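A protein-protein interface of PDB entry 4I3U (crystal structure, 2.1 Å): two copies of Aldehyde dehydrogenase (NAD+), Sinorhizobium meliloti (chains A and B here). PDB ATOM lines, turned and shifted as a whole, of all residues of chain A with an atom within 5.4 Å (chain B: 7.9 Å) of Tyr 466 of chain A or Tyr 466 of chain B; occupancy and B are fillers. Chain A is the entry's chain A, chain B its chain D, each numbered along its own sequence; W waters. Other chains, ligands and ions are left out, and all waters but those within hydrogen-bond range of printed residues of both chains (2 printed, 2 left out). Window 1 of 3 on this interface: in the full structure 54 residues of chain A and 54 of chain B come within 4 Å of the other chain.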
ATOM      1  N   ARG A 253      32.381  -5.016  13.800  1.00  0.00           N
ATOM      2  CA  ARG A 253      30.981  -4.782  14.076  1.00  0.00           C
ATOM      3  C   ARG A 253      30.272  -6.108  14.270  1.00  0.00           C
ATOM      4  O   ARG A 253      30.600  -7.102  13.628  1.00  0.00           O
ATOM      5  CB  ARG A 253      30.316  -3.991  12.974  1.00  0.00           C
ATOM      6  CG  ARG A 253      30.915  -2.621  12.859  1.00  0.00           C
ATOM      7  CD  ARG A 253      29.974  -1.673  12.029  1.00  0.00           C
ATOM      8  NE  ARG A 253      30.045  -2.013  10.638  1.00  0.00           N
ATOM      9  CZ  ARG A 253      30.685  -1.271   9.757  1.00  0.00           C
ATOM     10  NH1 ARG A 253      31.360  -0.207  10.124  1.00  0.00           N
ATOM     11  NH2 ARG A 253      30.705  -1.625   8.506  1.00  0.00           N
ATOM     12  N   GLN A 254      29.307  -6.122  15.175  1.00  0.00           N
ATOM     13  CA  GLN A 254      28.616  -7.348  15.536  1.00  0.00           C
ATOM     14  C   GLN A 254      27.146  -7.039  15.625  1.00  0.00           C
ATOM     15  O   GLN A 254      26.717  -6.076  16.285  1.00  0.00           O
ATOM     16  CB  GLN A 254      29.099  -7.872  16.885  1.00  0.00           C
ATOM     17  CG  GLN A 254      30.600  -8.116  16.996  1.00  0.00           C
ATOM     18  CD  GLN A 254      31.041  -8.244  18.439  1.00  0.00           C
ATOM     19  OE1 GLN A 254      30.259  -8.611  19.305  1.00  0.00           O
ATOM     20  NE2 GLN A 254      32.293  -7.932  18.698  1.00  0.00           N
ATOM     21  N   VAL A 255      26.353  -7.860  14.956  1.00  0.00           N
ATOM     22  CA  VAL A 255      24.907  -7.778  15.144  1.00  0.00           C
ATOM     23  C   VAL A 255      24.480  -9.109  15.737  1.00  0.00           C
ATOM     24  O   VAL A 255      24.498 -10.142  15.050  1.00  0.00           O
ATOM     25  CB  VAL A 255      24.190  -7.465  13.836  1.00  0.00           C
ATOM     26  CG1 VAL A 255      22.704  -7.526  14.005  1.00  0.00           C
ATOM     27  CG2 VAL A 255      24.619  -6.068  13.356  1.00  0.00           C
ATOM     28  N   GLU A 257      21.790 -11.452  17.741  1.00  0.00           N
ATOM     29  CA  GLU A 257      20.380 -11.696  17.996  1.00  0.00           C
ATOM     30  C   GLU A 257      20.252 -12.955  18.814  1.00  0.00           C
ATOM     31  O   GLU A 257      20.480 -14.040  18.315  1.00  0.00           O
ATOM     32  CB  GLU A 257      19.672 -11.901  16.685  1.00  0.00           C
ATOM     33  CG  GLU A 257      19.007 -10.646  16.272  1.00  0.00           C
ATOM     34  CD  GLU A 257      18.185 -10.141  17.394  1.00  0.00           C
ATOM     35  OE1 GLU A 257      17.455 -11.010  17.996  1.00  0.00           O
ATOM     36  OE2 GLU A 257      18.395  -8.921  17.721  1.00  0.00           O
ATOM     37  N   PHE A 456      13.916  -4.894  13.694  1.00  0.00           N
ATOM     38  CA  PHE A 456      13.769  -6.062  14.550  1.00  0.00           C
ATOM     39  C   PHE A 456      15.022  -6.232  15.383  1.00  0.00           C
ATOM     40  O   PHE A 456      16.135  -6.255  14.846  1.00  0.00           O
ATOM     41  CB  PHE A 456      13.526  -7.334  13.742  1.00  0.00           C
ATOM     42  CG  PHE A 456      13.507  -8.593  14.579  1.00  0.00           C
ATOM     43  CD1 PHE A 456      12.459  -8.853  15.444  1.00  0.00           C
ATOM     44  CD2 PHE A 456      14.528  -9.519  14.492  1.00  0.00           C
ATOM     45  CE1 PHE A 456      12.424 -10.035  16.208  1.00  0.00           C
ATOM     46  CE2 PHE A 456      14.512 -10.690  15.250  1.00  0.00           C
ATOM     47  CZ  PHE A 456      13.467 -10.938  16.121  1.00  0.00           C
ATOM     48  N   GLY A 457      14.842  -6.364  16.691  1.00  0.00           N
ATOM     49  CA  GLY A 457      15.962  -6.570  17.579  1.00  0.00           C
ATOM     50  C   GLY A 457      15.549  -6.311  19.011  1.00  0.00           C
ATOM     51  O   GLY A 457      14.647  -5.525  19.247  1.00  0.00           O
ATOM     52  N   GLY A 458      16.212  -6.982  19.947  1.00  0.00           N
ATOM     53  CA  GLY A 458      15.944  -6.834  21.371  1.00  0.00           C
ATOM     54  C   GLY A 458      17.034  -6.103  22.148  1.00  0.00           C
ATOM     55  O   GLY A 458      18.010  -5.581  21.592  1.00  0.00           O
ATOM     56  N   ASN A 464      22.555  -7.410  21.331  1.00  0.00           N
ATOM     57  CA  ASN A 464      23.520  -6.381  21.700  1.00  0.00           C
ATOM     58  C   ASN A 464      23.086  -4.966  21.334  1.00  0.00           C
ATOM     59  O   ASN A 464      23.856  -4.024  21.491  1.00  0.00           O
ATOM     60  CB  ASN A 464      24.931  -6.692  21.171  1.00  0.00           C
ATOM     61  CG  ASN A 464      25.020  -6.669  19.645  1.00  0.00           C
ATOM     62  OD1 ASN A 464      24.044  -6.879  18.951  1.00  0.00           O
ATOM     63  ND2 ASN A 464      26.212  -6.384  19.125  1.00  0.00           N
ATOM     64  N   GLY A 465      21.850  -4.823  20.848  1.00  0.00           N
ATOM     65  CA  GLY A 465      21.255  -3.509  20.655  1.00  0.00           C
ATOM     66  C   GLY A 465      21.232  -2.920  19.245  1.00  0.00           C
ATOM     67  O   GLY A 465      20.985  -1.747  19.072  1.00  0.00           O
ATOM     68  N   TYR A 466      21.485  -3.723  18.230  1.00  0.00           N
ATOM     69  CA  TYR A 466      21.364  -3.242  16.858  1.00  0.00           C
ATOM     70  C   TYR A 466      20.168  -3.882  16.201  1.00  0.00           C
ATOM     71  O   TYR A 466      19.813  -5.017  16.507  1.00  0.00           O
ATOM     72  CB  TYR A 466      22.637  -3.538  16.061  1.00  0.00           C
ATOM     73  CG  TYR A 466      23.853  -2.903  16.683  1.00  0.00           C
ATOM     74  CD1 TYR A 466      24.118  -1.536  16.490  1.00  0.00           C
ATOM     75  CD2 TYR A 466      24.720  -3.643  17.488  1.00  0.00           C
ATOM     76  CE1 TYR A 466      25.210  -0.928  17.076  1.00  0.00           C
ATOM     77  CE2 TYR A 466      25.826  -3.046  18.073  1.00  0.00           C
ATOM     78  CZ  TYR A 466      26.068  -1.685  17.852  1.00  0.00           C
ATOM     79  OH  TYR A 466      27.156  -1.071  18.422  1.00  0.00           O
ATOM     80  N   LYS A 467      19.536  -3.151  15.300  1.00  0.00           N
ATOM     81  CA  LYS A 467      18.344  -3.662  14.635  1.00  0.00           C
ATOM     82  C   LYS A 467      18.678  -4.445  13.385  1.00  0.00           C
ATOM     83  O   LYS A 467      19.701  -4.230  12.740  1.00  0.00           O
ATOM     84  CB  LYS A 467      17.355  -2.548  14.331  1.00  0.00           C
ATOM     85  CG  LYS A 467      16.761  -1.905  15.589  1.00  0.00           C
ATOM     86  CD  LYS A 467      15.863  -2.856  16.366  1.00  0.00           C
ATOM     87  CE  LYS A 467      15.274  -2.173  17.570  1.00  0.00           C
ATOM     88  NZ  LYS A 467      14.102  -2.927  18.117  1.00  0.00           N
ATOM     89  N   GLU A 468      17.806  -5.389  13.093  1.00  0.00           N
ATOM     90  CA  GLU A 468      17.874  -6.242  11.919  1.00  0.00           C
ATOM     91  C   GLU A 468      16.570  -6.026  11.150  1.00  0.00           C
ATOM     92  O   GLU A 468      15.831  -5.063  11.393  1.00  0.00           O
ATOM     93  CB  GLU A 468      17.845  -7.700  12.373  1.00  0.00           C
ATOM     94  CG  GLU A 468      19.129  -8.392  12.667  1.00  0.00           C
ATOM     95  CD  GLU A 468      18.917  -9.898  12.651  1.00  0.00           C
ATOM     96  OE1 GLU A 468      18.001 -10.365  13.353  1.00  0.00           O
ATOM     97  OE2 GLU A 468      19.633 -10.601  11.906  1.00  0.00           O
ATOM     98  N   ASP B 231      25.274   0.575  29.114  1.00  0.00           N
ATOM     99  CA  ASP B 231      24.680   0.020  27.900  1.00  0.00           C
ATOM    100  C   ASP B 231      25.538   0.354  26.690  1.00  0.00           C
ATOM    101  O   ASP B 231      25.541  -0.359  25.680  1.00  0.00           O
ATOM    102  CB  ASP B 231      23.274   0.582  27.688  1.00  0.00           C
ATOM    103  CG  ASP B 231      22.235  -0.154  28.474  1.00  0.00           C
ATOM    104  OD1 ASP B 231      22.571  -1.209  29.041  1.00  0.00           O
ATOM    105  OD2 ASP B 231      21.082   0.310  28.519  1.00  0.00           O
ATOM    106  N   LEU B 232      26.263   1.455  26.803  1.00  0.00           N
ATOM    107  CA  LEU B 232      27.044   1.954  25.696  1.00  0.00           C
ATOM    108  C   LEU B 232      28.315   2.665  26.182  1.00  0.00           C
ATOM    109  O   LEU B 232      28.276   3.491  27.092  1.00  0.00           O
ATOM    110  CB  LEU B 232      26.192   2.918  24.858  1.00  0.00           C
ATOM    111  CG  LEU B 232      26.824   3.466  23.566  1.00  0.00           C
ATOM    112  CD1 LEU B 232      25.786   3.658  22.483  1.00  0.00           C
ATOM    113  CD2 LEU B 232      27.499   4.794  23.846  1.00  0.00           C
ATOM    114  N   VAL B 233      29.436   2.325  25.556  1.00  0.00           N
ATOM    115  CA  VAL B 233      30.694   3.026  25.780  1.00  0.00           C
ATOM    116  C   VAL B 233      30.989   3.898  24.565  1.00  0.00           C
ATOM    117  O   VAL B 233      31.061   3.416  23.421  1.00  0.00           O
ATOM    118  CB  VAL B 233      31.868   2.083  26.004  1.00  0.00           C
ATOM    119  CG1 VAL B 233      33.185   2.904  26.145  1.00  0.00           C
ATOM    120  CG2 VAL B 233      31.631   1.207  27.229  1.00  0.00           C
ATOM    121  N   LYS B 252      28.604  -4.813  25.120  1.00  0.00           N
ATOM    122  CA  LYS B 252      28.128  -3.451  25.289  1.00  0.00           C
ATOM    123  C   LYS B 252      28.269  -2.816  23.936  1.00  0.00           C
ATOM    124  O   LYS B 252      29.201  -3.123  23.213  1.00  0.00           O
ATOM    125  CB  LYS B 252      28.948  -2.673  26.314  1.00  0.00           C
ATOM    126  CG  LYS B 252      28.832  -3.226  27.713  1.00  0.00           C
ATOM    127  CD  LYS B 252      29.707  -2.460  28.694  1.00  0.00           C
ATOM    128  CE  LYS B 252      29.638  -3.090  30.076  1.00  0.00           C
ATOM    129  NZ  LYS B 252      28.247  -3.118  30.607  1.00  0.00           N
ATOM    130  N   ARG B 253      27.338  -1.954  23.565  1.00  0.00           N
ATOM    131  CA  ARG B 253      27.532  -1.176  22.358  1.00  0.00           C
ATOM    132  C   ARG B 253      28.703  -0.261  22.546  1.00  0.00           C
ATOM    133  O   ARG B 253      28.949   0.234  23.635  1.00  0.00           O
ATOM    134  CB  ARG B 253      26.300  -0.369  22.032  1.00  0.00           C
ATOM    135  CG  ARG B 253      25.129  -1.210  21.674  1.00  0.00           C
ATOM    136  CD  ARG B 253      24.076  -0.387  20.944  1.00  0.00           C
ATOM    137  NE  ARG B 253      23.326   0.474  21.846  1.00  0.00           N
ATOM    138  CZ  ARG B 253      22.081   0.231  22.245  1.00  0.00           C
ATOM    139  NH1 ARG B 253      21.426  -0.832  21.824  1.00  0.00           N
ATOM    140  NH2 ARG B 253      21.476   1.065  23.050  1.00  0.00           N
ATOM    141  N   GLN B 254      29.464  -0.072  21.488  1.00  0.00           N
ATOM    142  CA  GLN B 254      30.688   0.726  21.576  1.00  0.00           C
ATOM    143  C   GLN B 254      30.746   1.647  20.382  1.00  0.00           C
ATOM    144  O   GLN B 254      30.527   1.233  19.235  1.00  0.00           O
ATOM    145  CB  GLN B 254      31.934  -0.175  21.542  1.00  0.00           C
ATOM    146  CG  GLN B 254      32.024  -1.210  22.651  1.00  0.00           C
ATOM    147  CD  GLN B 254      32.989  -2.319  22.294  1.00  0.00           C
ATOM    148  OE1 GLN B 254      33.948  -2.096  21.563  1.00  0.00           O
ATOM    149  NE2 GLN B 254      32.734  -3.523  22.792  1.00  0.00           N
ATOM    150  N   VAL B 255      31.053   2.900  20.633  1.00  0.00           N
ATOM    151  CA  VAL B 255      31.301   3.813  19.547  1.00  0.00           C
ATOM    152  C   VAL B 255      32.706   4.328  19.746  1.00  0.00           C
ATOM    153  O   VAL B 255      32.949   5.095  20.667  1.00  0.00           O
ATOM    154  CB  VAL B 255      30.305   5.020  19.564  1.00  0.00           C
ATOM    155  CG1 VAL B 255      30.720   6.047  18.515  1.00  0.00           C
ATOM    156  CG2 VAL B 255      28.878   4.532  19.297  1.00  0.00           C
ATOM    157  N   LEU B 256      33.624   3.866  18.898  1.00  0.00           N
ATOM    158  CA  LEU B 256      35.047   4.081  19.086  1.00  0.00           C
ATOM    159  C   LEU B 256      35.589   4.973  17.998  1.00  0.00           C
ATOM    160  O   LEU B 256      35.495   4.674  16.800  1.00  0.00           O
ATOM    161  CB  LEU B 256      35.814   2.770  19.101  1.00  0.00           C
ATOM    162  CG  LEU B 256      35.276   1.722  20.058  1.00  0.00           C
ATOM    163  CD1 LEU B 256      36.103   0.464  19.940  1.00  0.00           C
ATOM    164  CD2 LEU B 256      35.274   2.265  21.504  1.00  0.00           C
ATOM    165  N   GLU B 257      36.167   6.078  18.420  1.00  0.00           N
ATOM    166  CA  GLU B 257      36.717   7.070  17.507  1.00  0.00           C
ATOM    167  C   GLU B 257      38.211   7.170  17.745  1.00  0.00           C
ATOM    168  O   GLU B 257      38.668   7.679  18.772  1.00  0.00           O
ATOM    169  CB  GLU B 257      36.072   8.408  17.799  1.00  0.00           C
ATOM    170  CG  GLU B 257      34.979   8.677  16.839  1.00  0.00           C
ATOM    171  CD  GLU B 257      35.474   8.461  15.442  1.00  0.00           C
ATOM    172  OE1 GLU B 257      36.608   8.974  15.166  1.00  0.00           O
ATOM    173  OE2 GLU B 257      34.793   7.677  14.703  1.00  0.00           O
ATOM    174  N   PRO B 455      27.185  13.440   9.826  1.00  0.00           N
ATOM    175  CA  PRO B 455      27.694  12.131  10.262  1.00  0.00           C
ATOM    176  C   PRO B 455      29.216  12.115  10.234  1.00  0.00           C
ATOM    177  O   PRO B 455      29.812  12.496   9.240  1.00  0.00           O
ATOM    178  CB  PRO B 455      27.118  11.151   9.226  1.00  0.00           C
ATOM    179  CG  PRO B 455      25.925  11.839   8.632  1.00  0.00           C
ATOM    180  CD  PRO B 455      26.303  13.323   8.647  1.00  0.00           C
ATOM    181  N   PHE B 456      29.817  11.711  11.341  1.00  0.00           N
ATOM    182  CA  PHE B 456      31.267  11.799  11.513  1.00  0.00           C
ATOM    183  C   PHE B 456      31.795  10.478  12.044  1.00  0.00           C
ATOM    184  O   PHE B 456      31.298   9.963  13.047  1.00  0.00           O
ATOM    185  CB  PHE B 456      31.645  12.913  12.495  1.00  0.00           C
ATOM    186  CG  PHE B 456      33.121  12.939  12.822  1.00  0.00           C
ATOM    187  CD1 PHE B 456      34.043  13.312  11.861  1.00  0.00           C
ATOM    188  CD2 PHE B 456      33.584  12.545  14.068  1.00  0.00           C
ATOM    189  CE1 PHE B 456      35.408  13.311  12.131  1.00  0.00           C
ATOM    190  CE2 PHE B 456      34.943  12.530  14.351  1.00  0.00           C
ATOM    191  CZ  PHE B 456      35.851  12.921  13.395  1.00  0.00           C
ATOM    192  N   GLY B 457      32.805   9.935  11.377  1.00  0.00           N
ATOM    193  CA  GLY B 457      33.388   8.682  11.810  1.00  0.00           C
ATOM    194  C   GLY B 457      34.189   8.039  10.699  1.00  0.00           C
ATOM    195  O   GLY B 457      33.940   8.257   9.515  1.00  0.00           O
ATOM    196  N   GLY B 458      35.166   7.244  11.091  1.00  0.00           N
ATOM    197  CA  GLY B 458      36.058   6.626  10.134  1.00  0.00           C
ATOM    198  C   GLY B 458      35.898   5.124  10.057  1.00  0.00           C
ATOM    199  O   GLY B 458      35.038   4.537  10.730  1.00  0.00           O
ATOM    200  N   ILE B 459      36.747   4.520   9.234  1.00  0.00           N
ATOM    201  CA  ILE B 459      36.812   3.092   9.030  1.00  0.00           C
ATOM    202  C   ILE B 459      38.266   2.662   9.264  1.00  0.00           C
ATOM    203  O   ILE B 459      39.091   3.472   9.660  1.00  0.00           O
ATOM    204  CB  ILE B 459      36.381   2.765   7.600  1.00  0.00           C
ATOM    205  CG1 ILE B 459      37.277   3.482   6.602  1.00  0.00           C
ATOM    206  CG2 ILE B 459      34.948   3.232   7.362  1.00  0.00           C
ATOM    207  CD1 ILE B 459      37.010   3.082   5.178  1.00  0.00           C
ATOM    208  N   SER B 462      40.540   3.877  12.130  1.00  0.00           N
ATOM    209  CA  SER B 462      40.057   5.180  12.589  1.00  0.00           C
ATOM    210  C   SER B 462      38.800   5.115  13.436  1.00  0.00           C
ATOM    211  O   SER B 462      38.493   6.051  14.174  1.00  0.00           O
ATOM    212  CB  SER B 462      39.818   6.127  11.422  1.00  0.00           C
ATOM    213  OG  SER B 462      41.029   6.598  10.915  1.00  0.00           O
ATOM    214  N   GLY B 463      38.040   4.042  13.291  1.00  0.00           N
ATOM    215  CA  GLY B 463      36.912   3.821  14.162  1.00  0.00           C
ATOM    216  C   GLY B 463      36.332   2.451  13.899  1.00  0.00           C
ATOM    217  O   GLY B 463      36.665   1.838  12.878  1.00  0.00           O
ATOM    218  N   ASN B 464      35.466   1.981  14.800  1.00  0.00           N
ATOM    219  CA  ASN B 464      34.845   0.656  14.656  1.00  0.00           C
ATOM    220  C   ASN B 464      33.636   0.661  13.743  1.00  0.00           C
ATOM    221  O   ASN B 464      32.947  -0.345  13.636  1.00  0.00           O
ATOM    222  CB  ASN B 464      34.498   0.014  15.999  1.00  0.00           C
ATOM    223  CG  ASN B 464      33.475   0.826  16.809  1.00  0.00           C
ATOM    224  OD1 ASN B 464      33.355   2.040  16.654  1.00  0.00           O
ATOM    225  ND2 ASN B 464      32.739   0.141  17.683  1.00  0.00           N
ATOM    226  N   GLY B 465      33.381   1.793  13.090  1.00  0.00           N
ATOM    227  CA  GLY B 465      32.389   1.852  12.027  1.00  0.00           C
ATOM    228  C   GLY B 465      31.025   2.461  12.323  1.00  0.00           C
ATOM    229  O   GLY B 465      30.080   2.325  11.546  1.00  0.00           O
ATOM    230  N   TYR B 466      30.894   3.144  13.444  1.00  0.00           N
ATOM    231  CA  TYR B 466      29.648   3.823  13.758  1.00  0.00           C
ATOM    232  C   TYR B 466      29.824   5.331  13.668  1.00  0.00           C
ATOM    233  O   TYR B 466      30.885   5.859  13.947  1.00  0.00           O
ATOM    234  CB  TYR B 466      29.177   3.435  15.157  1.00  0.00           C
ATOM    235  CG  TYR B 466      28.937   1.946  15.304  1.00  0.00           C
ATOM    236  CD1 TYR B 466      27.769   1.351  14.812  1.00  0.00           C
ATOM    237  CD2 TYR B 466      29.897   1.126  15.894  1.00  0.00           C
ATOM    238  CE1 TYR B 466      27.549  -0.009  14.935  1.00  0.00           C
ATOM    239  CE2 TYR B 466      29.681  -0.248  16.032  1.00  0.00           C
ATOM    240  CZ  TYR B 466      28.497  -0.802  15.543  1.00  0.00           C
ATOM    241  OH  TYR B 466      28.283  -2.158  15.661  1.00  0.00           O
ATOM    242  N   LYS B 467      28.774   6.028  13.288  1.00  0.00           N
ATOM    243  CA  LYS B 467      28.879   7.470  13.144  1.00  0.00           C
ATOM    244  C   LYS B 467      28.548   8.214  14.422  1.00  0.00           C
ATOM    245  O   LYS B 467      27.865   7.708  15.326  1.00  0.00           O
ATOM    246  CB  LYS B 467      28.026   7.958  11.982  1.00  0.00           C
ATOM    247  CG  LYS B 467      28.513   7.397  10.634  1.00  0.00           C
ATOM    248  CD  LYS B 467      29.831   8.016  10.192  1.00  0.00           C
ATOM    249  CE  LYS B 467      30.239   7.468   8.822  1.00  0.00           C
ATOM    250  NZ  LYS B 467      31.335   8.251   8.130  1.00  0.00           N
ATOM    251  N   GLU B 468      29.087   9.416  14.486  1.00  0.00           N
ATOM    252  CA  GLU B 468      28.974  10.324  15.608  1.00  0.00           C
ATOM    253  C   GLU B 468      28.531  11.633  14.986  1.00  0.00           C
ATOM    254  O   GLU B 468      28.128  11.692  13.824  1.00  0.00           O
ATOM    255  CB  GLU B 468      30.353  10.618  16.213  1.00  0.00           C
ATOM    256  CG  GLU B 468      30.873   9.758  17.349  1.00  0.00           C
ATOM    257  CD  GLU B 468      32.008  10.473  18.079  1.00  0.00           C
ATOM    258  OE1 GLU B 468      32.951  10.951  17.391  1.00  0.00           O
ATOM    259  OE2 GLU B 468      31.937  10.619  19.331  1.00  0.00           O
ATOM    260  N   GLY B 469      28.720  12.706  15.747  1.00  0.00           N
ATOM    261  CA  GLY B 469      28.123  13.987  15.432  1.00  0.00           C
ATOM    262  C   GLY B 469      26.801  13.988  16.159  1.00  0.00           C
ATOM    263  O   GLY B 469      26.328  12.944  16.597  1.00  0.00           O
ATOM    264  N   GLU B 472      23.699  11.561  14.727  1.00  0.00           N
ATOM    265  CA  GLU B 472      23.981  10.136  14.828  1.00  0.00           C
ATOM    266  C   GLU B 472      24.276   9.694  16.260  1.00  0.00           C
ATOM    267  O   GLU B 472      23.943   8.586  16.644  1.00  0.00           O
ATOM    268  CB  GLU B 472      25.126   9.753  13.892  1.00  0.00           C
ATOM    269  CG  GLU B 472      24.757   9.959  12.410  1.00  0.00           C
ATOM    270  CD  GLU B 472      23.618   9.045  11.961  1.00  0.00           C
ATOM    271  OE1 GLU B 472      23.456   7.937  12.533  1.00  0.00           O
ATOM    272  OE2 GLU B 472      22.873   9.433  11.035  1.00  0.00           O
ATOM    273  N   SER B 476      22.315   6.843  18.254  1.00  0.00           N
ATOM    274  CA  SER B 476      23.197   5.844  18.814  1.00  0.00           C
ATOM    275  C   SER B 476      22.900   5.648  20.301  1.00  0.00           C
ATOM    276  O   SER B 476      23.075   4.550  20.853  1.00  0.00           O
ATOM    277  CB  SER B 476      24.625   6.334  18.634  1.00  0.00           C
ATOM    278  OG  SER B 476      25.512   5.305  18.864  1.00  0.00           O
ATOM    279  N   THR B 478      20.079   5.647  21.822  1.00  0.00           N
ATOM    280  CA  THR B 478      18.704   5.221  22.109  1.00  0.00           C
ATOM    281  C   THR B 478      18.448   3.813  21.618  1.00  0.00           C
ATOM    282  O   THR B 478      19.189   3.281  20.785  1.00  0.00           O
ATOM    283  CB  THR B 478      17.667   6.160  21.445  1.00  0.00           C
ATOM    284  OG1 THR B 478      17.870   6.173  20.026  1.00  0.00           O
ATOM    285  CG2 THR B 478      17.779   7.586  21.963  1.00  0.00           C
ATOM    286  N   ASN B 479      17.403   3.188  22.132  1.00  0.00           N
ATOM    287  CA  ASN B 479      16.911   1.956  21.536  1.00  0.00           C
ATOM    288  C   ASN B 479      15.661   2.298  20.734  1.00  0.00           C
ATOM    289  O   ASN B 479      14.837   3.085  21.187  1.00  0.00           O
ATOM    290  CB  ASN B 479      16.571   0.921  22.617  1.00  0.00           C
ATOM    291  CG  ASN B 479      17.785   0.452  23.336  1.00  0.00           C
ATOM    292  OD1 ASN B 479      18.832   0.082  22.698  1.00  0.00           O
ATOM    293  ND2 ASN B 479      17.693   0.469  24.682  1.00  0.00           N
HETATM  294  O   HOH W   1      32.882  -2.396  15.932  1.00  0.00           O
HETATM  295  O   HOH W   2      27.619   1.411  18.359  1.00  0.00           O
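O of Asn 464 of chain B touches CG of Arg 253 of chain A, 3.1 Å away. Tyr 466 of chain B touches Arg 253 of chain A (OH to CB, 3.8 Å). CG of Arg 253 of chain B touches O of Asn 464 of chain A (3.1 Å). Arg 253 of chain B touches Tyr 466 of chain A (CB to OH, 3.8 Å). Tyr 466 of chain A touches Gln 254 of chain B (OH to N, 3.97 Å).
Water W2 lies within hydrogen-bond range of the side-chain hydroxyl (OH) of Tyr 466 of chain A and the backbone carbonyl oxygen (O) of Gln 254 of chain B. Water W1 bridges the backbone carbonyl oxygen (O) of Asn 464 of chain B (3.1 Å) and the backbone NH (N) of Arg 253 of chain A (3.4 Å).
Of the 26 printed residues of chain B, 5 touch a printed residue of chain A. Printed residues of chain B that touch a printed residue of chain A: Arg 253, Gln 254, Asn 464, Gly 465 and Tyr 466. Hydrophobic or aromatic side chains of chain B within 4 Å of the printed part of chain A: Tyr 466. Along chain B the printed residues that touch a printed residue of chain A span positions 253 to 466. Of the 12 printed residues of chain A, 4 touch a printed residue of chain B. Among the printed residues, 8 pairs touch across the chains.
The backbone carbonyl oxygen of Gly 465 of chain B lies close to the guanidinium group of Arg 253 of chain A, at 3.2 Å. O of Gly 465 of chain A lies close to NH1 of Arg 253 of chain B, 2.9 Å away. OH of Tyr 466 of chain A lies close to OH of Tyr 466 of chain B, at 3.2 Å.
Gly 465 of chain A touches one residue of chain B. Of the printed residues of chain A, Gln 254 of chain B touches Tyr 466 (3.97 Å). Of the printed residues of chain A, Gly 465 of chain B touches Arg 253. Tyr 466 of chain B touches two residues of chain A.
Arg 253 of chain A touches Asn 464 of chain B, and with the chains exchanged Asn 464 of chain A touches Arg 253 of chain B. Arg 253 of chain A touches Tyr 466 of chain B, and with the chains exchanged Tyr 466 of chain A touches Arg 253 of chain B. Tyr 466 of chain A touches Gln 254 of chain B, but with the chains exchanged Gln 254 of chain A does not touch Tyr 466 of chain B (4.1 Å). Tyr 466 of chain B touches its own counterpart, Tyr 466 of chain A. 12 positions are printed for both chains. Of the 8 pairs that touch across the chains among the printed residues, 7 have their exchanged pair printed and touching as well.
ND2 of Asn 464 of chain A is in hydrogen-bond range of O of Gln 254 of chain A (2.9 Å). The backbone NH of Arg 253 of chain B is in hydrogen-bond range of the backbone carbonyl oxygen of Asp 231 of chain B, 3.2 Å away. The backbone carbonyl oxygen (O) of Arg 253 of chain B lies within hydrogen-bond range of the backbone NH (N) of Val 233 of chain B (2.9 Å). The guanidinium group (NH2) of Arg 253 of chain B lies within hydrogen-bond range of the side-chain amide oxygen (OD1) of Asn 479 of chain B (2.8 Å). O of Gln 254 of chain B lies within hydrogen-bond range of ND2 of Asn 464 of chain B. The side-chain amide oxygen (OD1) of Asn 464 of chain B sits at hydrogen-bond distance from the backbone NH (N) of Leu 256 of chain B, 2.9 Å away.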
